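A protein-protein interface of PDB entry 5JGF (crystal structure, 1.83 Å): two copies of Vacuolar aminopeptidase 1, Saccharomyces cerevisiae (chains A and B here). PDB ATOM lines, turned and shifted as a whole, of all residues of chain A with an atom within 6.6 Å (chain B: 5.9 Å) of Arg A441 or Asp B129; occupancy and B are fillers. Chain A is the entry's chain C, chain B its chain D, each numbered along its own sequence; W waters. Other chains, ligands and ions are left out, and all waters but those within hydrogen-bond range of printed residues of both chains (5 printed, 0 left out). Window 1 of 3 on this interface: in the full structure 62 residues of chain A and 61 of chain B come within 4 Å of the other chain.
The side-chain carboxylate (OD1) of Asp A242 sits at hydrogen-bond distance from the backbone NH (N) of Gln A244 (2.8 Å). The guanidinium group (NH2) of Arg B162 lies within salt-bridge range of the side-chain carboxylate (OD1) of Asp B129. The side-chain carboxylate (OD2) of Asp B129 is in hydrogen-bond range of the side-chain hydroxyl (OG) of Ser B165. The guanidinium group (NE) of Arg A130 lies within hydrogen-bond range of the backbone carbonyl oxygen (O) of Leu A126. The backbone carbonyl oxygen (O) of Lys A245 is in hydrogen-bond range of the guanidinium group (NH1) of Arg A441 (3.0 Å). The backbone NH of Ala A442 is in hydrogen-bond range of the backbone carbonyl oxygen of Ala A258 (3.0 Å).
Hydrophobic or aromatic side chains of chain A that line the printed part of chain B: Leu A126, Phe A257 and Ala A443. Among the printed residues, 19 pairs touch across the chains.
Among the printed residues, pairs that only touch across the chains: Arg A441 with Asp B129 (3.4 Å), Phe A257 with Arg B162 (3.4 Å), Ala A442 with Arg B162 (3.5 Å), Phe A257 with Asp B131 (3.6 Å), Thr A247 with Asp B131 (3.7 Å), Ser A436 with Pro B164 (3.8 Å), Ala A443 with Arg B162 (3.8 Å), Leu A126 with Asp B129 (3.9 Å), Ser A439 with Ser B165 (3.9 Å) and Gln A244 with Asp B131 (3.9 Å).
Asp B129 touches just these residues of chain A: Leu A126, Arg A130, Ser A436, Ser A439 and Arg A441. Printed residues of chain A within 4 Å of Asp B131: Gln A244 (3.9 Å), Thr A247 (3.7 Å), Phe A257 (3.6 Å) and Arg A441 (2.8 Å). Printed residues of chain A within 4 Å of Pro B164: Ser A436. Of the printed residues of chain A, Ser B165 touches Ser A436 (3.0 Å) and Ser A439 (3.9 Å). The nearest residue of chain B that does not touch Arg A441 is Arg B130 (5.4 Å).
Water W1 lies within hydrogen-bond range of OD2 of Asp B131 (2.6 Å) and OG1 of Thr A247 (3.0 Å). Water W5 lies within hydrogen-bond range of O of Ser B165 and N of Ser A436. Water W4 lies within hydrogen-bond range of O of Glu B125, NH2 of Arg A130 and O of Leu B128. Water W2 lies within hydrogen-bond range of N of Asp B131 and NE2 of Gln A244. Water W3 bridges NH2 of Arg B130 and O of Leu A126.
Arg B130 touches its own counterpart, Arg A130. Of the 19 pairs that touch across the chains among the printed residues, 1 has its exchanged pair printed and touching as well.
The side-chain carboxylate (OD1) of Asp B129 sits at hydrogen-bond distance from the side-chain hydroxyl (OG) of Ser A436 (3.3 Å). NE of Arg A130 lies close to NH2 of Arg B130, 3.5 Å away. The guanidinium group (NH1) of Arg A130 is in hydrogen-bond range of the backbone carbonyl oxygen (O) of Asp B129 (3.1 Å). The backbone carbonyl oxygen (O) of Leu B128 is in hydrogen-bond range of the guanidinium group (NH2) of Arg A130. The side-chain hydroxyl of Ser A436 lies within hydrogen-bond range of the guanidinium group of Arg B162, at 3.1 Å. OD2 of Asp B129 is in hydrogen-bond range of OG of Ser A439, 2.5 Å away. O of Arg A441 lies within hydrogen-bond range of NH2 of Arg B162, 2.8 Å away. OD2 of Asp B131 lies within salt-bridge range of NH1 of Arg A441 (2.8 Å). O of Ser B165 lies within hydrogen-bond range of OG of Ser A436 (3.0 Å).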
ATOM      1  N   LEU A 126      -9.274  13.757  10.587  1.00  0.00           N
ATOM      2  CA  LEU A 126      -8.846  13.007  11.760  1.00  0.00           C
ATOM      3  C   LEU A 126      -9.294  11.547  11.654  1.00  0.00           C
ATOM      4  O   LEU A 126      -8.728  10.672  12.308  1.00  0.00           O
ATOM      5  CB  LEU A 126      -9.403  13.642  13.040  1.00  0.00           C
ATOM      6  CG  LEU A 126      -8.897  15.056  13.357  1.00  0.00           C
ATOM      7  CD1 LEU A 126      -9.556  15.557  14.632  1.00  0.00           C
ATOM      8  CD2 LEU A 126      -7.382  15.049  13.527  1.00  0.00           C
ATOM      9  N   ARG A 130      -7.125   5.574   9.872  1.00  0.00           N
ATOM     10  CA  ARG A 130      -7.330   5.076  11.228  1.00  0.00           C
ATOM     11  C   ARG A 130      -7.899   3.666  11.079  1.00  0.00           C
ATOM     12  O   ARG A 130      -8.737   3.424  10.206  1.00  0.00           O
ATOM     13  CB  ARG A 130      -8.337   5.954  11.973  1.00  0.00           C
ATOM     14  CG  ARG A 130      -7.902   7.406  12.147  1.00  0.00           C
ATOM     15  CD  ARG A 130      -6.927   7.585  13.311  1.00  0.00           C
ATOM     16  NE  ARG A 130      -6.561   8.993  13.470  1.00  0.00           N
ATOM     17  CZ  ARG A 130      -5.898   9.490  14.508  1.00  0.00           C
ATOM     18  NH1 ARG A 130      -5.508   8.698  15.500  1.00  0.00           N
ATOM     19  NH2 ARG A 130      -5.642  10.789  14.565  1.00  0.00           N
ATOM     20  N   ASP A 242     -12.680   3.585  15.961  1.00  0.00           N
ATOM     21  CA  ASP A 242     -11.241   3.369  16.076  1.00  0.00           C
ATOM     22  C   ASP A 242     -10.989   2.196  17.025  1.00  0.00           C
ATOM     23  O   ASP A 242     -11.490   2.189  18.148  1.00  0.00           O
ATOM     24  CB  ASP A 242     -10.564   4.624  16.635  1.00  0.00           C
ATOM     25  CG  ASP A 242      -9.053   4.599  16.470  1.00  0.00           C
ATOM     26  OD1 ASP A 242      -8.471   3.496  16.389  1.00  0.00           O
ATOM     27  OD2 ASP A 242      -8.447   5.689  16.432  1.00  0.00           O
ATOM     28  N   VAL A 243     -10.214   1.212  16.579  1.00  0.00           N
ATOM     29  CA  VAL A 243      -9.921   0.057  17.423  1.00  0.00           C
ATOM     30  C   VAL A 243      -8.605   0.183  18.176  1.00  0.00           C
ATOM     31  O   VAL A 243      -8.164  -0.778  18.803  1.00  0.00           O
ATOM     32  CB  VAL A 243      -9.859  -1.258  16.616  1.00  0.00           C
ATOM     33  CG1 VAL A 243     -11.221  -1.581  16.041  1.00  0.00           C
ATOM     34  CG2 VAL A 243      -8.811  -1.151  15.526  1.00  0.00           C
ATOM     35  N   GLN A 244      -7.963   1.346  18.114  1.00  0.00           N
ATOM     36  CA  GLN A 244      -6.707   1.506  18.835  1.00  0.00           C
ATOM     37  C   GLN A 244      -7.000   1.662  20.321  1.00  0.00           C
ATOM     38  O   GLN A 244      -7.669   2.606  20.738  1.00  0.00           O
ATOM     39  CB  GLN A 244      -5.925   2.719  18.329  1.00  0.00           C
ATOM     40  CG  GLN A 244      -4.616   2.947  19.091  1.00  0.00           C
ATOM     41  CD  GLN A 244      -3.803   4.105  18.542  1.00  0.00           C
ATOM     42  OE1 GLN A 244      -4.354   5.057  17.999  1.00  0.00           O
ATOM     43  NE2 GLN A 244      -2.483   4.034  18.703  1.00  0.00           N
ATOM     44  N   LYS A 245      -6.501   0.722  21.118  1.00  0.00           N
ATOM     45  CA  LYS A 245      -6.722   0.755  22.560  1.00  0.00           C
ATOM     46  C   LYS A 245      -6.096   1.992  23.190  1.00  0.00           C
ATOM     47  O   LYS A 245      -5.052   2.468  22.741  1.00  0.00           O
ATOM     48  CB  LYS A 245      -6.140  -0.505  23.210  1.00  0.00           C
ATOM     49  CG  LYS A 245      -6.439  -0.633  24.699  1.00  0.00           C
ATOM     50  CD  LYS A 245      -5.950  -1.972  25.252  1.00  0.00           C
ATOM     51  CE  LYS A 245      -6.344  -2.128  26.715  1.00  0.00           C
ATOM     52  NZ  LYS A 245      -5.996  -3.474  27.256  1.00  0.00           N
ATOM     53  N   GLY A 246      -6.750   2.513  24.225  1.00  0.00           N
ATOM     54  CA  GLY A 246      -6.242   3.685  24.917  1.00  0.00           C
ATOM     55  C   GLY A 246      -4.897   3.395  25.559  1.00  0.00           C
ATOM     56  O   GLY A 246      -4.555   2.233  25.794  1.00  0.00           O
ATOM     57  N   THR A 247      -4.140   4.445  25.855  1.00  0.00           N
ATOM     58  CA  THR A 247      -2.822   4.286  26.450  1.00  0.00           C
ATOM     59  C   THR A 247      -2.482   5.424  27.399  1.00  0.00           C
ATOM     60  O   THR A 247      -2.935   6.553  27.217  1.00  0.00           O
ATOM     61  CB  THR A 247      -1.712   4.280  25.372  1.00  0.00           C
ATOM     62  OG1 THR A 247      -2.060   3.375  24.316  1.00  0.00           O
ATOM     63  CG2 THR A 247      -0.384   3.852  25.984  1.00  0.00           C
ATOM     64  N   PHE A 257      -4.508   8.683  26.650  1.00  0.00           N
ATOM     65  CA  PHE A 257      -4.941   8.862  25.268  1.00  0.00           C
ATOM     66  C   PHE A 257      -5.960   7.774  24.960  1.00  0.00           C
ATOM     67  O   PHE A 257      -5.680   6.590  25.149  1.00  0.00           O
ATOM     68  CB  PHE A 257      -3.761   8.717  24.296  1.00  0.00           C
ATOM     69  CG  PHE A 257      -2.581   9.600  24.616  1.00  0.00           C
ATOM     70  CD1 PHE A 257      -2.761  10.874  25.148  1.00  0.00           C
ATOM     71  CD2 PHE A 257      -1.288   9.174  24.332  1.00  0.00           C
ATOM     72  CE1 PHE A 257      -1.670  11.712  25.388  1.00  0.00           C
ATOM     73  CE2 PHE A 257      -0.188  10.006  24.567  1.00  0.00           C
ATOM     74  CZ  PHE A 257      -0.380  11.275  25.095  1.00  0.00           C
ATOM     75  N   ALA A 258      -7.139   8.166  24.488  1.00  0.00           N
ATOM     76  CA  ALA A 258      -8.174   7.189  24.172  1.00  0.00           C
ATOM     77  C   ALA A 258      -9.280   7.808  23.332  1.00  0.00           C
ATOM     78  O   ALA A 258      -9.496   9.019  23.359  1.00  0.00           O
ATOM     79  CB  ALA A 258      -8.768   6.610  25.467  1.00  0.00           C
ATOM     80  N   PRO A 259      -9.995   6.976  22.567  1.00  0.00           N
ATOM     81  CA  PRO A 259     -11.083   7.482  21.732  1.00  0.00           C
ATOM     82  C   PRO A 259     -12.379   7.603  22.522  1.00  0.00           C
ATOM     83  O   PRO A 259     -12.512   7.049  23.617  1.00  0.00           O
ATOM     84  CB  PRO A 259     -11.196   6.421  20.649  1.00  0.00           C
ATOM     85  CG  PRO A 259     -10.924   5.154  21.437  1.00  0.00           C
ATOM     86  CD  PRO A 259      -9.727   5.554  22.276  1.00  0.00           C
ATOM     87  N   ARG A 260     -13.312   8.361  21.962  1.00  0.00           N
ATOM     88  CA  ARG A 260     -14.639   8.520  22.534  1.00  0.00           C
ATOM     89  C   ARG A 260     -14.728   8.997  23.987  1.00  0.00           C
ATOM     90  O   ARG A 260     -15.617   8.572  24.725  1.00  0.00           O
ATOM     91  CB  ARG A 260     -15.381   7.186  22.350  1.00  0.00           C
ATOM     92  CG  ARG A 260     -15.301   6.653  20.900  1.00  0.00           C
ATOM     93  CD  ARG A 260     -15.974   5.292  20.711  1.00  0.00           C
ATOM     94  NE  ARG A 260     -15.271   4.175  21.351  1.00  0.00           N
ATOM     95  CZ  ARG A 260     -14.235   3.519  20.828  1.00  0.00           C
ATOM     96  NH1 ARG A 260     -13.684   2.510  21.504  1.00  0.00           N
ATOM     97  NH2 ARG A 260     -13.744   3.859  19.640  1.00  0.00           N
ATOM     98  N   LEU A 261     -13.826   9.890  24.393  1.00  0.00           N
ATOM     99  CA  LEU A 261     -13.837  10.416  25.760  1.00  0.00           C
ATOM    100  C   LEU A 261     -15.116  11.216  26.032  1.00  0.00           C
ATOM    101  O   LEU A 261     -15.689  11.143  27.110  1.00  0.00           O
ATOM    102  CB  LEU A 261     -12.603  11.298  26.003  1.00  0.00           C
ATOM    103  CG  LEU A 261     -11.222  10.634  25.966  1.00  0.00           C
ATOM    104  CD1 LEU A 261     -10.175  11.634  26.443  1.00  0.00           C
ATOM    105  CD2 LEU A 261     -11.205   9.396  26.861  1.00  0.00           C
ATOM    106  N   LEU A 435      -8.491  17.265  26.115  1.00  0.00           N
ATOM    107  CA  LEU A 435      -7.920  17.909  24.946  1.00  0.00           C
ATOM    108  C   LEU A 435      -8.562  17.237  23.742  1.00  0.00           C
ATOM    109  O   LEU A 435      -9.075  16.118  23.846  1.00  0.00           O
ATOM    110  CB  LEU A 435      -6.408  17.659  24.875  1.00  0.00           C
ATOM    111  CG  LEU A 435      -5.458  18.421  25.794  1.00  0.00           C
ATOM    112  CD1 LEU A 435      -4.056  17.826  25.665  1.00  0.00           C
ATOM    113  CD2 LEU A 435      -5.448  19.897  25.411  1.00  0.00           C
ATOM    114  N   SER A 436      -8.543  17.933  22.611  1.00  0.00           N
ATOM    115  CA  SER A 436      -9.042  17.400  21.352  1.00  0.00           C
ATOM    116  C   SER A 436     -10.446  16.813  21.348  1.00  0.00           C
ATOM    117  O   SER A 436     -10.677  15.759  20.754  1.00  0.00           O
ATOM    118  CB  SER A 436      -8.050  16.350  20.850  1.00  0.00           C
ATOM    119  OG  SER A 436      -6.720  16.834  20.960  1.00  0.00           O
ATOM    120  N   HIS A 438     -13.932  15.674  20.344  1.00  0.00           N
ATOM    121  CA  HIS A 438     -14.469  15.298  19.038  1.00  0.00           C
ATOM    122  C   HIS A 438     -13.463  14.745  18.035  1.00  0.00           C
ATOM    123  O   HIS A 438     -13.803  14.490  16.882  1.00  0.00           O
ATOM    124  CB  HIS A 438     -15.262  16.451  18.415  1.00  0.00           C
ATOM    125  CG  HIS A 438     -16.592  16.681  19.067  1.00  0.00           C
ATOM    126  ND1 HIS A 438     -17.574  17.468  18.504  1.00  0.00           N
ATOM    127  CD2 HIS A 438     -17.099  16.226  20.238  1.00  0.00           C
ATOM    128  CE1 HIS A 438     -18.630  17.487  19.300  1.00  0.00           C
ATOM    129  NE2 HIS A 438     -18.367  16.742  20.357  1.00  0.00           N
ATOM    130  N   SER A 439     -12.221  14.566  18.460  1.00  0.00           N
ATOM    131  CA  SER A 439     -11.238  13.959  17.576  1.00  0.00           C
ATOM    132  C   SER A 439     -11.575  12.472  17.639  1.00  0.00           C
ATOM    133  O   SER A 439     -12.410  12.063  18.442  1.00  0.00           O
ATOM    134  CB  SER A 439      -9.818  14.158  18.103  1.00  0.00           C
ATOM    135  OG  SER A 439      -8.921  13.312  17.398  1.00  0.00           O
ATOM    136  N   ILE A 440     -10.939  11.660  16.805  1.00  0.00           N
ATOM    137  CA  ILE A 440     -11.204  10.229  16.862  1.00  0.00           C
ATOM    138  C   ILE A 440     -10.410   9.644  18.041  1.00  0.00           C
ATOM    139  O   ILE A 440     -10.714   8.562  18.538  1.00  0.00           O
ATOM    140  CB  ILE A 440     -10.808   9.531  15.543  1.00  0.00           C
ATOM    141  CG1 ILE A 440     -11.392   8.115  15.519  1.00  0.00           C
ATOM    142  CG2 ILE A 440      -9.291   9.528  15.381  1.00  0.00           C
ATOM    143  CD1 ILE A 440     -11.143   7.369  14.220  1.00  0.00           C
ATOM    144  N   ARG A 441      -9.395  10.376  18.489  1.00  0.00           N
ATOM    145  CA  ARG A 441      -8.578   9.940  19.623  1.00  0.00           C
ATOM    146  C   ARG A 441      -8.192  11.176  20.429  1.00  0.00           C
ATOM    147  O   ARG A 441      -7.368  11.987  19.993  1.00  0.00           O
ATOM    148  CB  ARG A 441      -7.321   9.210  19.139  1.00  0.00           C
ATOM    149  CG  ARG A 441      -6.572   8.476  20.250  1.00  0.00           C
ATOM    150  CD  ARG A 441      -5.419   7.668  19.671  1.00  0.00           C
ATOM    151  NE  ARG A 441      -4.620   6.965  20.677  1.00  0.00           N
ATOM    152  CZ  ARG A 441      -4.980   5.835  21.285  1.00  0.00           C
ATOM    153  NH1 ARG A 441      -4.168   5.276  22.174  1.00  0.00           N
ATOM    154  NH2 ARG A 441      -6.146   5.267  21.015  1.00  0.00           N
ATOM    155  N   ALA A 442      -8.792  11.312  21.608  1.00  0.00           N
ATOM    156  CA  ALA A 442      -8.553  12.468  22.459  1.00  0.00           C
ATOM    157  C   ALA A 442      -7.610  12.191  23.619  1.00  0.00           C
ATOM    158  O   ALA A 442      -6.981  11.134  23.687  1.00  0.00           O
ATOM    159  CB  ALA A 442      -9.889  13.006  22.978  1.00  0.00           C
ATOM    160  N   ALA A 443      -7.514  13.148  24.534  1.00  0.00           N
ATOM    161  CA  ALA A 443      -6.630  12.992  25.677  1.00  0.00           C
ATOM    162  C   ALA A 443      -7.097  13.766  26.895  1.00  0.00           C
ATOM    163  O   ALA A 443      -7.757  14.796  26.777  1.00  0.00           O
ATOM    164  CB  ALA A 443      -5.221  13.441  25.301  1.00  0.00           C
ATOM    165  N   GLU B 125      -2.223  17.470   9.352  1.00  0.00           N
ATOM    166  CA  GLU B 125      -3.359  16.923  10.069  1.00  0.00           C
ATOM    167  C   GLU B 125      -3.312  15.424  10.338  1.00  0.00           C
ATOM    168  O   GLU B 125      -3.911  14.953  11.302  1.00  0.00           O
ATOM    169  CB  GLU B 125      -4.652  17.319   9.355  1.00  0.00           C
ATOM    170  CG  GLU B 125      -5.114  18.714   9.775  1.00  0.00           C
ATOM    171  CD  GLU B 125      -6.043  19.369   8.779  1.00  0.00           C
ATOM    172  OE1 GLU B 125      -5.553  19.822   7.721  1.00  0.00           O
ATOM    173  OE2 GLU B 125      -7.260  19.431   9.059  1.00  0.00           O
ATOM    174  N   TRP B 127      -0.798  13.880  11.357  1.00  0.00           N
ATOM    175  CA  TRP B 127       0.069  13.697  12.516  1.00  0.00           C
ATOM    176  C   TRP B 127      -0.572  14.157  13.819  1.00  0.00           C
ATOM    177  O   TRP B 127      -0.004  13.987  14.901  1.00  0.00           O
ATOM    178  CB  TRP B 127       1.404  14.421  12.307  1.00  0.00           C
ATOM    179  CG  TRP B 127       2.385  13.602  11.516  1.00  0.00           C
ATOM    180  CD1 TRP B 127       2.347  13.333  10.175  1.00  0.00           C
ATOM    181  CD2 TRP B 127       3.520  12.894  12.035  1.00  0.00           C
ATOM    182  NE1 TRP B 127       3.387  12.498   9.830  1.00  0.00           N
ATOM    183  CE2 TRP B 127       4.120  12.215  10.951  1.00  0.00           C
ATOM    184  CE3 TRP B 127       4.085  12.766  13.313  1.00  0.00           C
ATOM    185  CZ2 TRP B 127       5.264  11.417  11.105  1.00  0.00           C
ATOM    186  CZ3 TRP B 127       5.222  11.973  13.465  1.00  0.00           C
ATOM    187  CH2 TRP B 127       5.796  11.309  12.366  1.00  0.00           C
ATOM    188  N   LEU B 128      -1.762  14.737  13.719  1.00  0.00           N
ATOM    189  CA  LEU B 128      -2.463  15.197  14.910  1.00  0.00           C
ATOM    190  C   LEU B 128      -3.120  14.026  15.626  1.00  0.00           C
ATOM    191  O   LEU B 128      -3.593  13.082  14.994  1.00  0.00           O
ATOM    192  CB  LEU B 128      -3.562  16.196  14.544  1.00  0.00           C
ATOM    193  CG  LEU B 128      -3.159  17.518  13.895  1.00  0.00           C
ATOM    194  CD1 LEU B 128      -4.419  18.298  13.545  1.00  0.00           C
ATOM    195  CD2 LEU B 128      -2.278  18.313  14.839  1.00  0.00           C
ATOM    196  N   ASP B 129      -3.143  14.097  16.951  1.00  0.00           N
ATOM    197  CA  ASP B 129      -3.794  13.076  17.756  1.00  0.00           C
ATOM    198  C   ASP B 129      -3.320  11.658  17.479  1.00  0.00           C
ATOM    199  O   ASP B 129      -4.120  10.722  17.403  1.00  0.00           O
ATOM    200  CB  ASP B 129      -5.308  13.191  17.564  1.00  0.00           C
ATOM    201  CG  ASP B 129      -5.822  14.586  17.886  1.00  0.00           C
ATOM    202  OD1 ASP B 129      -5.082  15.340  18.547  1.00  0.00           O
ATOM    203  OD2 ASP B 129      -6.956  14.931  17.488  1.00  0.00           O
ATOM    204  N   ARG B 130      -2.009  11.514  17.332  1.00  0.00           N
ATOM    205  CA  ARG B 130      -1.371  10.223  17.103  1.00  0.00           C
ATOM    206  C   ARG B 130      -0.424  10.020  18.290  1.00  0.00           C
ATOM    207  O   ARG B 130       0.216  10.974  18.742  1.00  0.00           O
ATOM    208  CB  ARG B 130      -0.570  10.255  15.797  1.00  0.00           C
ATOM    209  CG  ARG B 130      -1.410  10.514  14.542  1.00  0.00           C
ATOM    210  CD  ARG B 130      -2.146   9.264  14.071  1.00  0.00           C
ATOM    211  NE  ARG B 130      -2.912   9.523  12.853  1.00  0.00           N
ATOM    212  CZ  ARG B 130      -3.471   8.582  12.100  1.00  0.00           C
ATOM    213  NH1 ARG B 130      -3.357   7.300  12.432  1.00  0.00           N
ATOM    214  NH2 ARG B 130      -4.138   8.920  11.005  1.00  0.00           N
ATOM    215  N   ASP B 131      -0.347   8.793  18.802  1.00  0.00           N
ATOM    216  CA  ASP B 131       0.528   8.480  19.935  1.00  0.00           C
ATOM    217  C   ASP B 131       1.967   8.446  19.430  1.00  0.00           C
ATOM    218  O   ASP B 131       2.332   7.558  18.657  1.00  0.00           O
ATOM    219  CB  ASP B 131       0.173   7.108  20.518  1.00  0.00           C
ATOM    220  CG  ASP B 131      -1.190   7.078  21.193  1.00  0.00           C
ATOM    221  OD1 ASP B 131      -1.987   8.026  21.019  1.00  0.00           O
ATOM    222  OD2 ASP B 131      -1.466   6.084  21.897  1.00  0.00           O
ATOM    223  N   ARG B 162       2.424  13.861  21.855  1.00  0.00           N
ATOM    224  CA  ARG B 162       1.173  13.862  21.113  1.00  0.00           C
ATOM    225  C   ARG B 162       0.916  15.312  20.719  1.00  0.00           C
ATOM    226  O   ARG B 162       1.037  16.208  21.553  1.00  0.00           O
ATOM    227  CB  ARG B 162       0.025  13.333  21.982  1.00  0.00           C
ATOM    228  CG  ARG B 162      -1.357  13.377  21.320  1.00  0.00           C
ATOM    229  CD  ARG B 162      -2.417  12.739  22.225  1.00  0.00           C
ATOM    230  NE  ARG B 162      -3.775  12.814  21.682  1.00  0.00           N
ATOM    231  CZ  ARG B 162      -4.484  13.935  21.589  1.00  0.00           C
ATOM    232  NH1 ARG B 162      -3.968  15.087  22.003  1.00  0.00           N
ATOM    233  NH2 ARG B 162      -5.711  13.908  21.090  1.00  0.00           N
ATOM    234  N   ILE B 163       0.598  15.537  19.447  1.00  0.00           N
ATOM    235  CA  ILE B 163       0.309  16.879  18.940  1.00  0.00           C
ATOM    236  C   ILE B 163      -1.215  16.973  18.977  1.00  0.00           C
ATOM    237  O   ILE B 163      -1.906  16.382  18.148  1.00  0.00           O
ATOM    238  CB  ILE B 163       0.811  17.045  17.495  1.00  0.00           C
ATOM    239  CG1 ILE B 163       2.287  16.628  17.412  1.00  0.00           C
ATOM    240  CG2 ILE B 163       0.640  18.499  17.049  1.00  0.00           C
ATOM    241  CD1 ILE B 163       2.841  16.558  16.003  1.00  0.00           C
ATOM    242  N   PRO B 164      -1.754  17.740  19.934  1.00  0.00           N
ATOM    243  CA  PRO B 164      -3.196  17.922  20.130  1.00  0.00           C
ATOM    244  C   PRO B 164      -3.975  18.812  19.178  1.00  0.00           C
ATOM    245  O   PRO B 164      -3.679  19.997  19.039  1.00  0.00           O
ATOM    246  CB  PRO B 164      -3.266  18.441  21.558  1.00  0.00           C
ATOM    247  CG  PRO B 164      -2.083  19.354  21.610  1.00  0.00           C
ATOM    248  CD  PRO B 164      -0.991  18.535  20.917  1.00  0.00           C
ATOM    249  N   SER B 165      -4.992  18.241  18.539  1.00  0.00           N
ATOM    250  CA  SER B 165      -5.836  19.019  17.645  1.00  0.00           C
ATOM    251  C   SER B 165      -6.685  19.918  18.538  1.00  0.00           C
ATOM    252  O   SER B 165      -6.914  19.603  19.709  1.00  0.00           O
ATOM    253  CB  SER B 165      -6.755  18.102  16.829  1.00  0.00           C
ATOM    254  OG  SER B 165      -7.652  17.388  17.670  1.00  0.00           O
HETATM  255  O   HOH W   1      -0.305   3.727  21.854  1.00  0.00           O
HETATM  256  O   HOH W   2      -0.768   6.195  17.603  1.00  0.00           O
HETATM  257  O   HOH W   3      -5.968  11.302  10.424  1.00  0.00           O
HETATM  258  O   HOH W   4      -4.972  12.502  12.275  1.00  0.00           O
HETATM  259  O   HOH W   5      -7.351  20.542  22.263  1.00  0.00           O
